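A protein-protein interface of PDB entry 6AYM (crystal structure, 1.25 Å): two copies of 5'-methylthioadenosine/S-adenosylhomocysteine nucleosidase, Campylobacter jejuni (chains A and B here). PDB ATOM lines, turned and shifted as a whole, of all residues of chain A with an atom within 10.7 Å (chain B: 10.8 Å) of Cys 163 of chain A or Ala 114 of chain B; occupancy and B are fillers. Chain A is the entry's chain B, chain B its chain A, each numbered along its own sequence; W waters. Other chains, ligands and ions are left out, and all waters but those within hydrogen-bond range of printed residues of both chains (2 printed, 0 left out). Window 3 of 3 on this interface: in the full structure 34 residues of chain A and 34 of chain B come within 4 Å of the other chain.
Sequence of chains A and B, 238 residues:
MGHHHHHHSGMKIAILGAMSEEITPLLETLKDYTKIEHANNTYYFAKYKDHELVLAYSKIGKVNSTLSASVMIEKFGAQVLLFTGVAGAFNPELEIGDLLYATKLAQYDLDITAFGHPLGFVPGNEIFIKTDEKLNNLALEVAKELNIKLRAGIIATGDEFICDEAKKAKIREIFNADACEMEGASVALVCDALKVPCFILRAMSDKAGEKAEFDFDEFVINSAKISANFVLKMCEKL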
ATOM      1  N   GLY A  88     -17.169  21.889  29.359  1.00  0.00           N
ATOM      2  CA  GLY A  88     -17.516  20.654  28.661  1.00  0.00           C
ATOM      3  C   GLY A  88     -16.284  19.770  28.555  1.00  0.00           C
ATOM      4  O   GLY A  88     -15.226  20.239  28.157  1.00  0.00           O
ATOM      5  N   ALA A  89     -16.405  18.500  28.933  1.00  0.00           N
ATOM      6  CA  ALA A  89     -15.288  17.565  28.887  1.00  0.00           C
ATOM      7  C   ALA A  89     -15.065  17.028  27.476  1.00  0.00           C
ATOM      8  O   ALA A  89     -16.029  16.657  26.792  1.00  0.00           O
ATOM      9  CB  ALA A  89     -15.526  16.418  29.854  1.00  0.00           C
ATOM     10  N   PHE A  90     -13.811  17.021  27.038  1.00  0.00           N
ATOM     11  CA  PHE A  90     -13.391  16.420  25.766  1.00  0.00           C
ATOM     12  C   PHE A  90     -12.623  15.129  25.923  1.00  0.00           C
ATOM     13  O   PHE A  90     -12.654  14.269  25.012  1.00  0.00           O
ATOM     14  CB  PHE A  90     -12.446  17.362  25.007  1.00  0.00           C
ATOM     15  CG  PHE A  90     -13.094  18.567  24.401  1.00  0.00           C
ATOM     16  CD1 PHE A  90     -14.471  18.789  24.425  1.00  0.00           C
ATOM     17  CD2 PHE A  90     -12.278  19.490  23.753  1.00  0.00           C
ATOM     18  CE1 PHE A  90     -15.010  19.899  23.797  1.00  0.00           C
ATOM     19  CE2 PHE A  90     -12.828  20.600  23.138  1.00  0.00           C
ATOM     20  CZ  PHE A  90     -14.183  20.807  23.175  1.00  0.00           C
ATOM     21  N   TYR A 108      -8.903  28.620  21.173  1.00  0.00           N
ATOM     22  CA  TYR A 108      -9.025  27.798  19.944  1.00  0.00           C
ATOM     23  C   TYR A 108      -9.536  28.598  18.742  1.00  0.00           C
ATOM     24  O   TYR A 108      -9.374  28.147  17.604  1.00  0.00           O
ATOM     25  CB  TYR A 108      -9.888  26.534  20.157  1.00  0.00           C
ATOM     26  CG  TYR A 108     -11.342  26.823  20.476  1.00  0.00           C
ATOM     27  CD1 TYR A 108     -12.226  27.215  19.477  1.00  0.00           C
ATOM     28  CD2 TYR A 108     -11.837  26.700  21.767  1.00  0.00           C
ATOM     29  CE1 TYR A 108     -13.542  27.497  19.762  1.00  0.00           C
ATOM     30  CE2 TYR A 108     -13.161  26.959  22.060  1.00  0.00           C
ATOM     31  CZ  TYR A 108     -14.008  27.385  21.057  1.00  0.00           C
ATOM     32  OH  TYR A 108     -15.329  27.667  21.331  1.00  0.00           O
ATOM     33  N   GLY A 158     -12.934  29.535  23.938  1.00  0.00           N
ATOM     34  CA  GLY A 158     -13.362  30.292  22.790  1.00  0.00           C
ATOM     35  C   GLY A 158     -14.779  30.763  22.976  1.00  0.00           C
ATOM     36  O   GLY A 158     -15.453  30.381  23.905  1.00  0.00           O
ATOM     37  N   ASP A 159     -15.214  31.625  22.068  1.00  0.00           N
ATOM     38  CA  ASP A 159     -16.497  32.322  22.213  1.00  0.00           C
ATOM     39  C   ASP A 159     -17.695  31.608  21.582  1.00  0.00           C
ATOM     40  O   ASP A 159     -18.751  32.203  21.414  1.00  0.00           O
ATOM     41  CB  ASP A 159     -16.362  33.756  21.687  1.00  0.00           C
ATOM     42  CG  ASP A 159     -15.899  34.721  22.755  1.00  0.00           C
ATOM     43  OD1 ASP A 159     -16.052  34.406  23.962  1.00  0.00           O
ATOM     44  OD2 ASP A 159     -15.445  35.827  22.377  1.00  0.00           O
ATOM     45  N   GLU A 160     -17.529  30.329  21.242  1.00  0.00           N
ATOM     46  CA  GLU A 160     -18.640  29.501  20.809  1.00  0.00           C
ATOM     47  C   GLU A 160     -18.993  28.479  21.867  1.00  0.00           C
ATOM     48  O   GLU A 160     -18.117  27.888  22.491  1.00  0.00           O
ATOM     49  CB  GLU A 160     -18.238  28.777  19.524  1.00  0.00           C
ATOM     50  CG  GLU A 160     -19.336  27.967  18.845  1.00  0.00           C
ATOM     51  CD  GLU A 160     -18.862  27.239  17.592  1.00  0.00           C
ATOM     52  OE1 GLU A 160     -17.743  27.493  17.115  1.00  0.00           O
ATOM     53  OE2 GLU A 160     -19.635  26.384  17.078  1.00  0.00           O
ATOM     54  N   PHE A 161     -20.290  28.249  22.068  1.00  0.00           N
ATOM     55  CA  PHE A 161     -20.724  27.073  22.812  1.00  0.00           C
ATOM     56  C   PHE A 161     -20.818  25.949  21.787  1.00  0.00           C
ATOM     57  O   PHE A 161     -21.740  25.920  20.969  1.00  0.00           O
ATOM     58  CB  PHE A 161     -22.065  27.301  23.497  1.00  0.00           C
ATOM     59  CG  PHE A 161     -22.473  26.164  24.382  1.00  0.00           C
ATOM     60  CD1 PHE A 161     -22.169  26.182  25.734  1.00  0.00           C
ATOM     61  CD2 PHE A 161     -23.149  25.069  23.859  1.00  0.00           C
ATOM     62  CE1 PHE A 161     -22.550  25.132  26.560  1.00  0.00           C
ATOM     63  CE2 PHE A 161     -23.515  24.002  24.672  1.00  0.00           C
ATOM     64  CZ  PHE A 161     -23.221  24.043  26.026  1.00  0.00           C
ATOM     65  N   ILE A 162     -19.848  25.042  21.820  1.00  0.00           N
ATOM     66  CA  ILE A 162     -19.717  24.032  20.768  1.00  0.00           C
ATOM     67  C   ILE A 162     -20.607  22.824  21.046  1.00  0.00           C
ATOM     68  O   ILE A 162     -20.549  22.241  22.131  1.00  0.00           O
ATOM     69  CB  ILE A 162     -18.253  23.576  20.590  1.00  0.00           C
ATOM     70  CG1 ILE A 162     -17.374  24.776  20.203  1.00  0.00           C
ATOM     71  CG2 ILE A 162     -18.132  22.480  19.516  1.00  0.00           C
ATOM     72  CD1 ILE A 162     -15.901  24.514  20.379  1.00  0.00           C
ATOM     73  N   CYS A 163     -21.412  22.470  20.045  1.00  0.00           N
ATOM     74  CA  CYS A 163     -22.206  21.231  20.043  1.00  0.00           C
ATOM     75  C   CYS A 163     -21.745  20.206  19.000  1.00  0.00           C
ATOM     76  O   CYS A 163     -22.134  19.039  19.077  1.00  0.00           O
ATOM     77  CB  CYS A 163     -23.673  21.568  19.809  1.00  0.00           C
ATOM     78  SG  CYS A 163     -24.331  22.705  21.041  1.00  0.00           S
ATOM     79  N   ASP A 164     -20.929  20.637  18.037  1.00  0.00           N
ATOM     80  CA  ASP A 164     -20.449  19.777  16.959  1.00  0.00           C
ATOM     81  C   ASP A 164     -19.354  18.848  17.499  1.00  0.00           C
ATOM     82  O   ASP A 164     -18.269  19.309  17.868  1.00  0.00           O
ATOM     83  CB  ASP A 164     -19.919  20.655  15.819  1.00  0.00           C
ATOM     84  CG  ASP A 164     -19.574  19.869  14.577  1.00  0.00           C
ATOM     85  OD1 ASP A 164     -20.160  20.149  13.511  1.00  0.00           O
ATOM     86  OD2 ASP A 164     -18.722  18.973  14.654  1.00  0.00           O
ATOM     87  N   GLU A 165     -19.638  17.547  17.528  1.00  0.00           N
ATOM     88  CA  GLU A 165     -18.694  16.551  18.050  1.00  0.00           C
ATOM     89  C   GLU A 165     -17.375  16.501  17.286  1.00  0.00           C
ATOM     90  O   GLU A 165     -16.311  16.325  17.894  1.00  0.00           O
ATOM     91  CB  GLU A 165     -19.336  15.149  18.081  1.00  0.00           C
ATOM     92  CG  GLU A 165     -20.430  14.991  19.128  1.00  0.00           C
ATOM     93  CD  GLU A 165     -19.948  15.278  20.539  1.00  0.00           C
ATOM     94  OE1 GLU A 165     -18.818  14.860  20.878  1.00  0.00           O
ATOM     95  OE2 GLU A 165     -20.688  15.945  21.308  1.00  0.00           O
ATOM     96  N   ALA A 166     -17.438  16.663  15.965  1.00  0.00           N
ATOM     97  CA  ALA A 166     -16.231  16.709  15.141  1.00  0.00           C
ATOM     98  C   ALA A 166     -15.357  17.912  15.515  1.00  0.00           C
ATOM     99  O   ALA A 166     -14.135  17.788  15.563  1.00  0.00           O
ATOM    100  CB  ALA A 166     -16.586  16.733  13.658  1.00  0.00           C
ATOM    101  N   LYS A 167     -15.979  19.062  15.799  1.00  0.00           N
ATOM    102  CA  LYS A 167     -15.220  20.250  16.206  1.00  0.00           C
ATOM    103  C   LYS A 167     -14.542  20.038  17.562  1.00  0.00           C
ATOM    104  O   LYS A 167     -13.381  20.416  17.734  1.00  0.00           O
ATOM    105  CB  LYS A 167     -16.095  21.504  16.230  1.00  0.00           C
ATOM    106  CG  LYS A 167     -15.312  22.767  16.591  1.00  0.00           C
ATOM    107  CD  LYS A 167     -15.983  24.031  16.080  1.00  0.00           C
ATOM    108  CE  LYS A 167     -15.133  25.255  16.391  1.00  0.00           C
ATOM    109  NZ  LYS A 167     -15.590  26.450  15.621  1.00  0.00           N
ATOM    110  N   LYS A 168     -15.251  19.413  18.498  1.00  0.00           N
ATOM    111  CA  LYS A 168     -14.678  19.067  19.802  1.00  0.00           C
ATOM    112  C   LYS A 168     -13.432  18.180  19.633  1.00  0.00           C
ATOM    113  O   LYS A 168     -12.390  18.424  20.236  1.00  0.00           O
ATOM    114  CB  LYS A 168     -15.702  18.357  20.680  1.00  0.00           C
ATOM    115  CG  LYS A 168     -16.917  19.200  21.048  1.00  0.00           C
ATOM    116  CD  LYS A 168     -17.873  18.427  21.920  1.00  0.00           C
ATOM    117  CE  LYS A 168     -19.174  19.178  22.148  1.00  0.00           C
ATOM    118  NZ  LYS A 168     -20.051  18.448  23.111  1.00  0.00           N
ATOM    119  N   ALA A 169     -13.552  17.155  18.799  1.00  0.00           N
ATOM    120  CA  ALA A 169     -12.425  16.265  18.516  1.00  0.00           C
ATOM    121  C   ALA A 169     -11.241  17.007  17.903  1.00  0.00           C
ATOM    122  O   ALA A 169     -10.090  16.744  18.237  1.00  0.00           O
ATOM    123  CB  ALA A 169     -12.865  15.124  17.606  1.00  0.00           C
ATOM    124  N   LYS A 170     -11.524  17.948  17.017  1.00  0.00           N
ATOM    125  CA  LYS A 170     -10.477  18.716  16.359  1.00  0.00           C
ATOM    126  C   LYS A 170      -9.742  19.618  17.350  1.00  0.00           C
ATOM    127  O   LYS A 170      -8.517  19.719  17.311  1.00  0.00           O
ATOM    128  CB  LYS A 170     -11.053  19.547  15.203  1.00  0.00           C
ATOM    129  CG  LYS A 170     -10.009  20.094  14.243  1.00  0.00           C
ATOM    130  CD  LYS A 170      -9.409  19.011  13.356  1.00  0.00           C
ATOM    131  CE  LYS A 170      -8.158  19.504  12.660  1.00  0.00           C
ATOM    132  NZ  LYS A 170      -7.580  18.433  11.804  1.00  0.00           N
ATOM    133  N   ILE A 171     -10.491  20.275  18.235  1.00  0.00           N
ATOM    134  CA  ILE A 171      -9.880  21.138  19.252  1.00  0.00           C
ATOM    135  C   ILE A 171      -9.030  20.285  20.200  1.00  0.00           C
ATOM    136  O   ILE A 171      -7.926  20.666  20.546  1.00  0.00           O
ATOM    137  CB  ILE A 171     -10.948  21.922  20.023  1.00  0.00           C
ATOM    138  CG1 ILE A 171     -11.648  22.911  19.091  1.00  0.00           C
ATOM    139  CG2 ILE A 171     -10.345  22.674  21.203  1.00  0.00           C
ATOM    140  CD1 ILE A 171     -12.947  23.453  19.645  1.00  0.00           C
ATOM    141  N   CYS A 180     -13.364  22.434  27.631  1.00  0.00           N
ATOM    142  CA  CYS A 180     -13.579  23.607  26.828  1.00  0.00           C
ATOM    143  C   CYS A 180     -14.605  24.527  27.472  1.00  0.00           C
ATOM    144  O   CYS A 180     -15.618  24.072  28.007  1.00  0.00           O
ATOM    145  CB  CYS A 180     -14.020  23.110  25.468  1.00  0.00           C
ATOM    146  SG  CYS A 180     -14.212  24.336  24.200  1.00  0.00           S
ATOM    147  N   MET A 182     -15.634  29.221  27.825  1.00  0.00           N
ATOM    148  CA  MET A 182     -15.680  30.509  27.131  1.00  0.00           C
ATOM    149  C   MET A 182     -14.943  31.639  27.843  1.00  0.00           C
ATOM    150  O   MET A 182     -14.971  32.749  27.340  1.00  0.00           O
ATOM    151  CB  MET A 182     -17.143  30.894  26.903  1.00  0.00           C
ATOM    152  CG  MET A 182     -17.911  29.910  26.041  1.00  0.00           C
ATOM    153  SD  MET A 182     -19.655  30.299  25.808  1.00  0.00           S
ATOM    154  CE  MET A 182     -19.578  31.752  24.773  1.00  0.00           C
ATOM    155  N   ASP A 206     -20.629  18.541  31.065  1.00  0.00           N
ATOM    156  CA  ASP A 206     -21.067  17.819  29.887  1.00  0.00           C
ATOM    157  C   ASP A 206     -19.916  16.916  29.459  1.00  0.00           C
ATOM    158  O   ASP A 206     -18.742  17.211  29.748  1.00  0.00           O
ATOM    159  CB  ASP A 206     -21.478  18.813  28.798  1.00  0.00           C
ATOM    160  CG  ASP A 206     -22.052  18.135  27.581  1.00  0.00           C
ATOM    161  OD1 ASP A 206     -23.227  17.685  27.613  1.00  0.00           O
ATOM    162  OD2 ASP A 206     -21.336  18.049  26.553  1.00  0.00           O
ATOM    163  N   LYS A 207     -20.244  15.780  28.850  1.00  0.00           N
ATOM    164  CA  LYS A 207     -19.222  14.882  28.299  1.00  0.00           C
ATOM    165  C   LYS A 207     -19.415  14.797  26.800  1.00  0.00           C
ATOM    166  O   LYS A 207     -20.546  14.686  26.316  1.00  0.00           O
ATOM    167  CB  LYS A 207     -19.256  13.491  28.949  1.00  0.00           C
ATOM    168  CG  LYS A 207     -18.251  12.540  28.329  1.00  0.00           C
ATOM    169  CD  LYS A 207     -17.912  11.365  29.230  1.00  0.00           C
ATOM    170  CE  LYS A 207     -16.792  10.535  28.614  1.00  0.00           C
ATOM    171  NZ  LYS A 207     -16.271   9.497  29.546  1.00  0.00           N
ATOM    172  N   ALA A 208     -18.299  14.822  26.061  1.00  0.00           N
ATOM    173  CA  ALA A 208     -18.325  14.656  24.607  1.00  0.00           C
ATOM    174  C   ALA A 208     -18.904  13.278  24.256  1.00  0.00           C
ATOM    175  O   ALA A 208     -18.409  12.251  24.729  1.00  0.00           O
ATOM    176  CB  ALA A 208     -16.934  14.812  24.013  1.00  0.00           C
ATOM    177  N   GLY A 209     -19.974  13.277  23.464  1.00  0.00           N
ATOM    178  CA  GLY A 209     -20.573  12.028  22.962  1.00  0.00           C
ATOM    179  C   GLY A 209     -21.501  11.284  23.917  1.00  0.00           C
ATOM    180  O   GLY A 209     -21.919  10.164  23.610  1.00  0.00           O
ATOM    181  N   GLU A 210     -21.856  11.920  25.039  1.00  0.00           N
ATOM    182  CA  GLU A 210     -22.929  11.426  25.912  1.00  0.00           C
ATOM    183  C   GLU A 210     -24.096  12.401  25.922  1.00  0.00           C
ATOM    184  O   GLU A 210     -23.909  13.602  26.158  1.00  0.00           O
ATOM    185  CB  GLU A 210     -22.443  11.265  27.349  1.00  0.00           C
ATOM    186  CG  GLU A 210     -21.546  10.077  27.594  1.00  0.00           C
ATOM    187  CD  GLU A 210     -21.359   9.755  29.076  1.00  0.00           C
ATOM    188  OE1 GLU A 210     -21.586  10.636  29.949  1.00  0.00           O
ATOM    189  OE2 GLU A 210     -20.978   8.602  29.369  1.00  0.00           O
ATOM    190  N   LYS A 211     -25.303  11.880  25.695  1.00  0.00           N
ATOM    191  CA  LYS A 211     -26.532  12.618  25.990  1.00  0.00           C
ATOM    192  C   LYS A 211     -26.597  12.817  27.504  1.00  0.00           C
ATOM    193  O   LYS A 211     -26.397  11.861  28.254  1.00  0.00           O
ATOM    194  CB  LYS A 211     -27.761  11.848  25.503  1.00  0.00           C
ATOM    195  N   LEU B 110     -19.060  35.470  18.578  1.00  0.00           N
ATOM    196  CA  LEU B 110     -19.645  35.256  19.900  1.00  0.00           C
ATOM    197  C   LEU B 110     -20.965  34.537  19.674  1.00  0.00           C
ATOM    198  O   LEU B 110     -21.911  35.130  19.158  1.00  0.00           O
ATOM    199  CB  LEU B 110     -19.809  36.591  20.634  1.00  0.00           C
ATOM    200  CG  LEU B 110     -20.343  36.539  22.060  1.00  0.00           C
ATOM    201  CD1 LEU B 110     -19.516  35.634  22.959  1.00  0.00           C
ATOM    202  CD2 LEU B 110     -20.435  37.942  22.657  1.00  0.00           C
ATOM    203  N   ASP B 111     -20.994  33.255  20.022  1.00  0.00           N
ATOM    204  CA  ASP B 111     -22.015  32.341  19.474  1.00  0.00           C
ATOM    205  C   ASP B 111     -22.531  31.401  20.547  1.00  0.00           C
ATOM    206  O   ASP B 111     -21.914  30.382  20.839  1.00  0.00           O
ATOM    207  CB  ASP B 111     -21.404  31.557  18.297  1.00  0.00           C
ATOM    208  CG  ASP B 111     -22.380  30.580  17.637  1.00  0.00           C
ATOM    209  OD1 ASP B 111     -23.475  30.327  18.184  1.00  0.00           O
ATOM    210  OD2 ASP B 111     -22.012  30.066  16.564  1.00  0.00           O
ATOM    211  N   ILE B 112     -23.684  31.739  21.117  1.00  0.00           N
ATOM    212  CA  ILE B 112     -24.449  30.793  21.943  1.00  0.00           C
ATOM    213  C   ILE B 112     -25.814  30.579  21.274  1.00  0.00           C
ATOM    214  O   ILE B 112     -26.852  30.453  21.937  1.00  0.00           O
ATOM    215  CB  ILE B 112     -24.520  31.227  23.423  1.00  0.00           C
ATOM    216  CG1 ILE B 112     -25.147  32.607  23.597  1.00  0.00           C
ATOM    217  CG2 ILE B 112     -23.120  31.226  24.034  1.00  0.00           C
ATOM    218  CD1 ILE B 112     -25.465  32.926  25.050  1.00  0.00           C
ATOM    219  N   THR B 113     -25.789  30.499  19.948  1.00  0.00           N
ATOM    220  CA  THR B 113     -27.001  30.282  19.144  1.00  0.00           C
ATOM    221  C   THR B 113     -27.631  28.913  19.430  1.00  0.00           C
ATOM    222  O   THR B 113     -28.822  28.730  19.194  1.00  0.00           O
ATOM    223  CB  THR B 113     -26.724  30.388  17.626  1.00  0.00           C
ATOM    224  OG1 THR B 113     -25.778  29.392  17.221  1.00  0.00           O
ATOM    225  CG2 THR B 113     -26.212  31.771  17.226  1.00  0.00           C
ATOM    226  N   ALA B 114     -26.855  27.969  19.964  1.00  0.00           N
ATOM    227  CA  ALA B 114     -27.391  26.676  20.426  1.00  0.00           C
ATOM    228  C   ALA B 114     -28.528  26.815  21.435  1.00  0.00           C
ATOM    229  O   ALA B 114     -29.375  25.917  21.544  1.00  0.00           O
ATOM    230  CB  ALA B 114     -26.275  25.824  21.014  1.00  0.00           C
ATOM    231  N   PHE B 115     -28.560  27.919  22.179  1.00  0.00           N
ATOM    232  CA  PHE B 115     -29.608  28.190  23.168  1.00  0.00           C
ATOM    233  C   PHE B 115     -30.715  29.120  22.666  1.00  0.00           C
ATOM    234  O   PHE B 115     -31.476  29.647  23.475  1.00  0.00           O
ATOM    235  CB  PHE B 115     -28.979  28.754  24.440  1.00  0.00           C
ATOM    236  CG  PHE B 115     -28.055  27.791  25.120  1.00  0.00           C
ATOM    237  CD1 PHE B 115     -28.568  26.798  25.953  1.00  0.00           C
ATOM    238  CD2 PHE B 115     -26.677  27.863  24.932  1.00  0.00           C
ATOM    239  CE1 PHE B 115     -27.725  25.899  26.584  1.00  0.00           C
ATOM    240  CE2 PHE B 115     -25.833  26.969  25.562  1.00  0.00           C
ATOM    241  CZ  PHE B 115     -26.355  25.987  26.390  1.00  0.00           C
ATOM    242  N   GLY B 116     -30.816  29.304  21.350  1.00  0.00           N
ATOM    243  CA  GLY B 116     -31.896  30.084  20.749  1.00  0.00           C
ATOM    244  C   GLY B 116     -31.665  31.584  20.668  1.00  0.00           C
ATOM    245  O   GLY B 116     -32.591  32.344  20.390  1.00  0.00           O
ATOM    246  N   HIS B 117     -30.429  32.028  20.914  1.00  0.00           N
ATOM    247  CA  HIS B 117     -30.056  33.431  20.787  1.00  0.00           C
ATOM    248  C   HIS B 117     -29.585  33.737  19.372  1.00  0.00           C
ATOM    249  O   HIS B 117     -29.110  32.852  18.652  1.00  0.00           O
ATOM    250  CB  HIS B 117     -28.918  33.768  21.748  1.00  0.00           C
ATOM    251  CG  HIS B 117     -29.231  33.481  23.182  1.00  0.00           C
ATOM    252  ND1 HIS B 117     -30.164  34.195  23.905  1.00  0.00           N
ATOM    253  CD2 HIS B 117     -28.741  32.539  24.022  1.00  0.00           C
ATOM    254  CE1 HIS B 117     -30.225  33.706  25.129  1.00  0.00           C
ATOM    255  NE2 HIS B 117     -29.369  32.710  25.227  1.00  0.00           N
ATOM    256  N   PRO B 118     -29.701  35.008  18.960  1.00  0.00           N
ATOM    257  CA  PRO B 118     -29.078  35.409  17.705  1.00  0.00           C
ATOM    258  C   PRO B 118     -27.548  35.447  17.827  1.00  0.00           C
ATOM    259  O   PRO B 118     -27.002  35.604  18.931  1.00  0.00           O
ATOM    260  CB  PRO B 118     -29.641  36.811  17.445  1.00  0.00           C
ATOM    261  CG  PRO B 118     -30.158  37.296  18.744  1.00  0.00           C
ATOM    262  CD  PRO B 118     -30.391  36.124  19.639  1.00  0.00           C
ATOM    263  N   LEU B 119     -26.868  35.287  16.695  1.00  0.00           N
ATOM    264  CA  LEU B 119     -25.416  35.373  16.664  1.00  0.00           C
ATOM    265  C   LEU B 119     -24.959  36.727  17.189  1.00  0.00           C
ATOM    266  O   LEU B 119     -25.520  37.764  16.821  1.00  0.00           O
ATOM    267  CB  LEU B 119     -24.898  35.134  15.247  1.00  0.00           C
ATOM    268  CG  LEU B 119     -23.385  34.989  15.073  1.00  0.00           C
ATOM    269  CD1 LEU B 119     -22.872  33.773  15.838  1.00  0.00           C
ATOM    270  CD2 LEU B 119     -23.065  34.896  13.593  1.00  0.00           C
ATOM    271  N   GLY B 120     -23.944  36.698  18.049  1.00  0.00           N
ATOM    272  CA  GLY B 120     -23.378  37.901  18.641  1.00  0.00           C
ATOM    273  C   GLY B 120     -23.964  38.304  19.974  1.00  0.00           C
ATOM    274  O   GLY B 120     -23.413  39.190  20.638  1.00  0.00           O
ATOM    275  N   PHE B 121     -25.057  37.660  20.384  1.00  0.00           N
ATOM    276  CA  PHE B 121     -25.763  38.023  21.618  1.00  0.00           C
ATOM    277  C   PHE B 121     -25.395  37.101  22.772  1.00  0.00           C
ATOM    278  O   PHE B 121     -25.424  35.890  22.613  1.00  0.00           O
ATOM    279  CB  PHE B 121     -27.285  37.930  21.413  1.00  0.00           C
ATOM    280  CG  PHE B 121     -28.091  38.269  22.647  1.00  0.00           C
ATOM    281  CD1 PHE B 121     -28.414  39.590  22.941  1.00  0.00           C
ATOM    282  CD2 PHE B 121     -28.500  37.279  23.522  1.00  0.00           C
ATOM    283  CE1 PHE B 121     -29.153  39.911  24.072  1.00  0.00           C
ATOM    284  CE2 PHE B 121     -29.235  37.593  24.656  1.00  0.00           C
ATOM    285  CZ  PHE B 121     -29.557  38.906  24.926  1.00  0.00           C
ATOM    286  N   VAL B 122     -25.133  37.689  23.941  1.00  0.00           N
ATOM    287  CA  VAL B 122     -25.124  36.931  25.193  1.00  0.00           C
ATOM    288  C   VAL B 122     -25.965  37.682  26.227  1.00  0.00           C
ATOM    289  O   VAL B 122     -25.935  38.912  26.261  1.00  0.00           O
ATOM    290  CB  VAL B 122     -23.701  36.689  25.755  1.00  0.00           C
ATOM    291  CG1 VAL B 122     -22.918  35.786  24.808  1.00  0.00           C
ATOM    292  CG2 VAL B 122     -22.932  37.988  26.009  1.00  0.00           C
ATOM    293  N   PRO B 123     -26.726  36.931  27.064  1.00  0.00           N
ATOM    294  CA  PRO B 123     -27.480  37.595  28.127  1.00  0.00           C
ATOM    295  C   PRO B 123     -26.570  38.442  28.981  1.00  0.00           C
ATOM    296  O   PRO B 123     -25.485  37.981  29.368  1.00  0.00           O
ATOM    297  CB  PRO B 123     -28.035  36.434  28.952  1.00  0.00           C
ATOM    298  CG  PRO B 123     -28.125  35.308  27.996  1.00  0.00           C
ATOM    299  CD  PRO B 123     -26.997  35.483  27.026  1.00  0.00           C
HETATM  300  O   HOH W   1     -22.105  27.174  16.337  1.00  0.00           O
HETATM  301  O   HOH W   2     -23.808  27.928  20.117  1.00  0.00           O
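O of Asp 159 of chain A lies within hydrogen-bond range of N of Asp 111 of chain B (2.8 Å). O of Asp 111 of chain B sits at hydrogen-bond distance from N of Phe 161 of chain A (2.9 Å).
The backbone carbonyl oxygen (O) of Leu 110 of chain B is in hydrogen-bond range of the backbone NH (N) of Gly 120 of chain B (2.8 Å). OD1 of Asp 111 of chain B is in hydrogen-bond range of OG1 of Thr 113 of chain B (2.7 Å). OH of Tyr 108 of chain A sits at hydrogen-bond distance from O of Glu 160 of chain A (3.0 Å). NZ of Lys 167 of chain A lies within salt-bridge range of OE1 of Glu 160 of chain A (2.8 Å).
O of Asp 159 of chain A touches CA of Leu 110 of chain B, 3.5 Å away. Glu 160 of chain A touches Asp 111 of chain B. Phe 161 of chain A touches Phe 115 of chain B. SG of Cys 163 of chain A touches CB of Ala 114 of chain B (3.7 Å). CE of Met 182 of chain A touches CG2 of Ile 112 of chain B, 3.7 Å away.
Of chain B, only Ala 114 comes within 4 Å of Cys 163 of chain A. Ala 114 of chain B touches one residue of chain A. Of the printed residues of chain B, Phe 161 of chain A touches Asp 111 (2.9 Å) and Phe 115 (3.7 Å). No residue of chain B comes within 4 Å of Ile 162 of chain A. No residue of chain B comes within 4 Å of Asp 164 of chain A. No residue of chain B comes within 4 Å of Glu 165 of chain A. No residue of chain A comes within 4 Å of Thr 113 of chain B. Of chain A, only Phe 161 comes within 4 Å of Phe 115 of chain B. Printed residues of chain A within 4 Å of Leu 110 of chain B: Asp 159. Printed residues of chain B within 4 Å of Met 182 of chain A: Ile 112 (3.7 Å). Of the printed residues of chain B, Asp 159 of chain A touches Leu 110 and Asp 111. Of the printed residues of chain B, Glu 160 of chain A touches Asp 111.
Of the 14 printed residues of chain B, 5 touch a printed residue of chain A. Of the 26 printed residues of chain A, 5 touch a printed residue of chain B. Printed residues of chain A that touch a printed residue of chain B: Asp 159, Glu 160, Phe 161, Cys 163 and Met 182. Hydrophobic or aromatic side chains of chain A that line the printed part of chain B: Phe 161 and Met 182.
No position is printed for both chains. Of the 7 pairs that touch across the chains among the printed residues, none has its exchanged pair printed and touching as well.
Water W1 lies within hydrogen-bond range of OE2 of Glu 160 of chain A (2.7 Å) and OD2 of Asp 111 of chain B (2.9 Å). Water W2 lies within hydrogen-bond range of the backbone carbonyl oxygen (O) of Phe 161 of chain A, the backbone NH (N) of Ala 114 of chain B, the side-chain carboxylate (OD1) of Asp 111 of chain B and the backbone NH (N) of Thr 113 of chain B.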
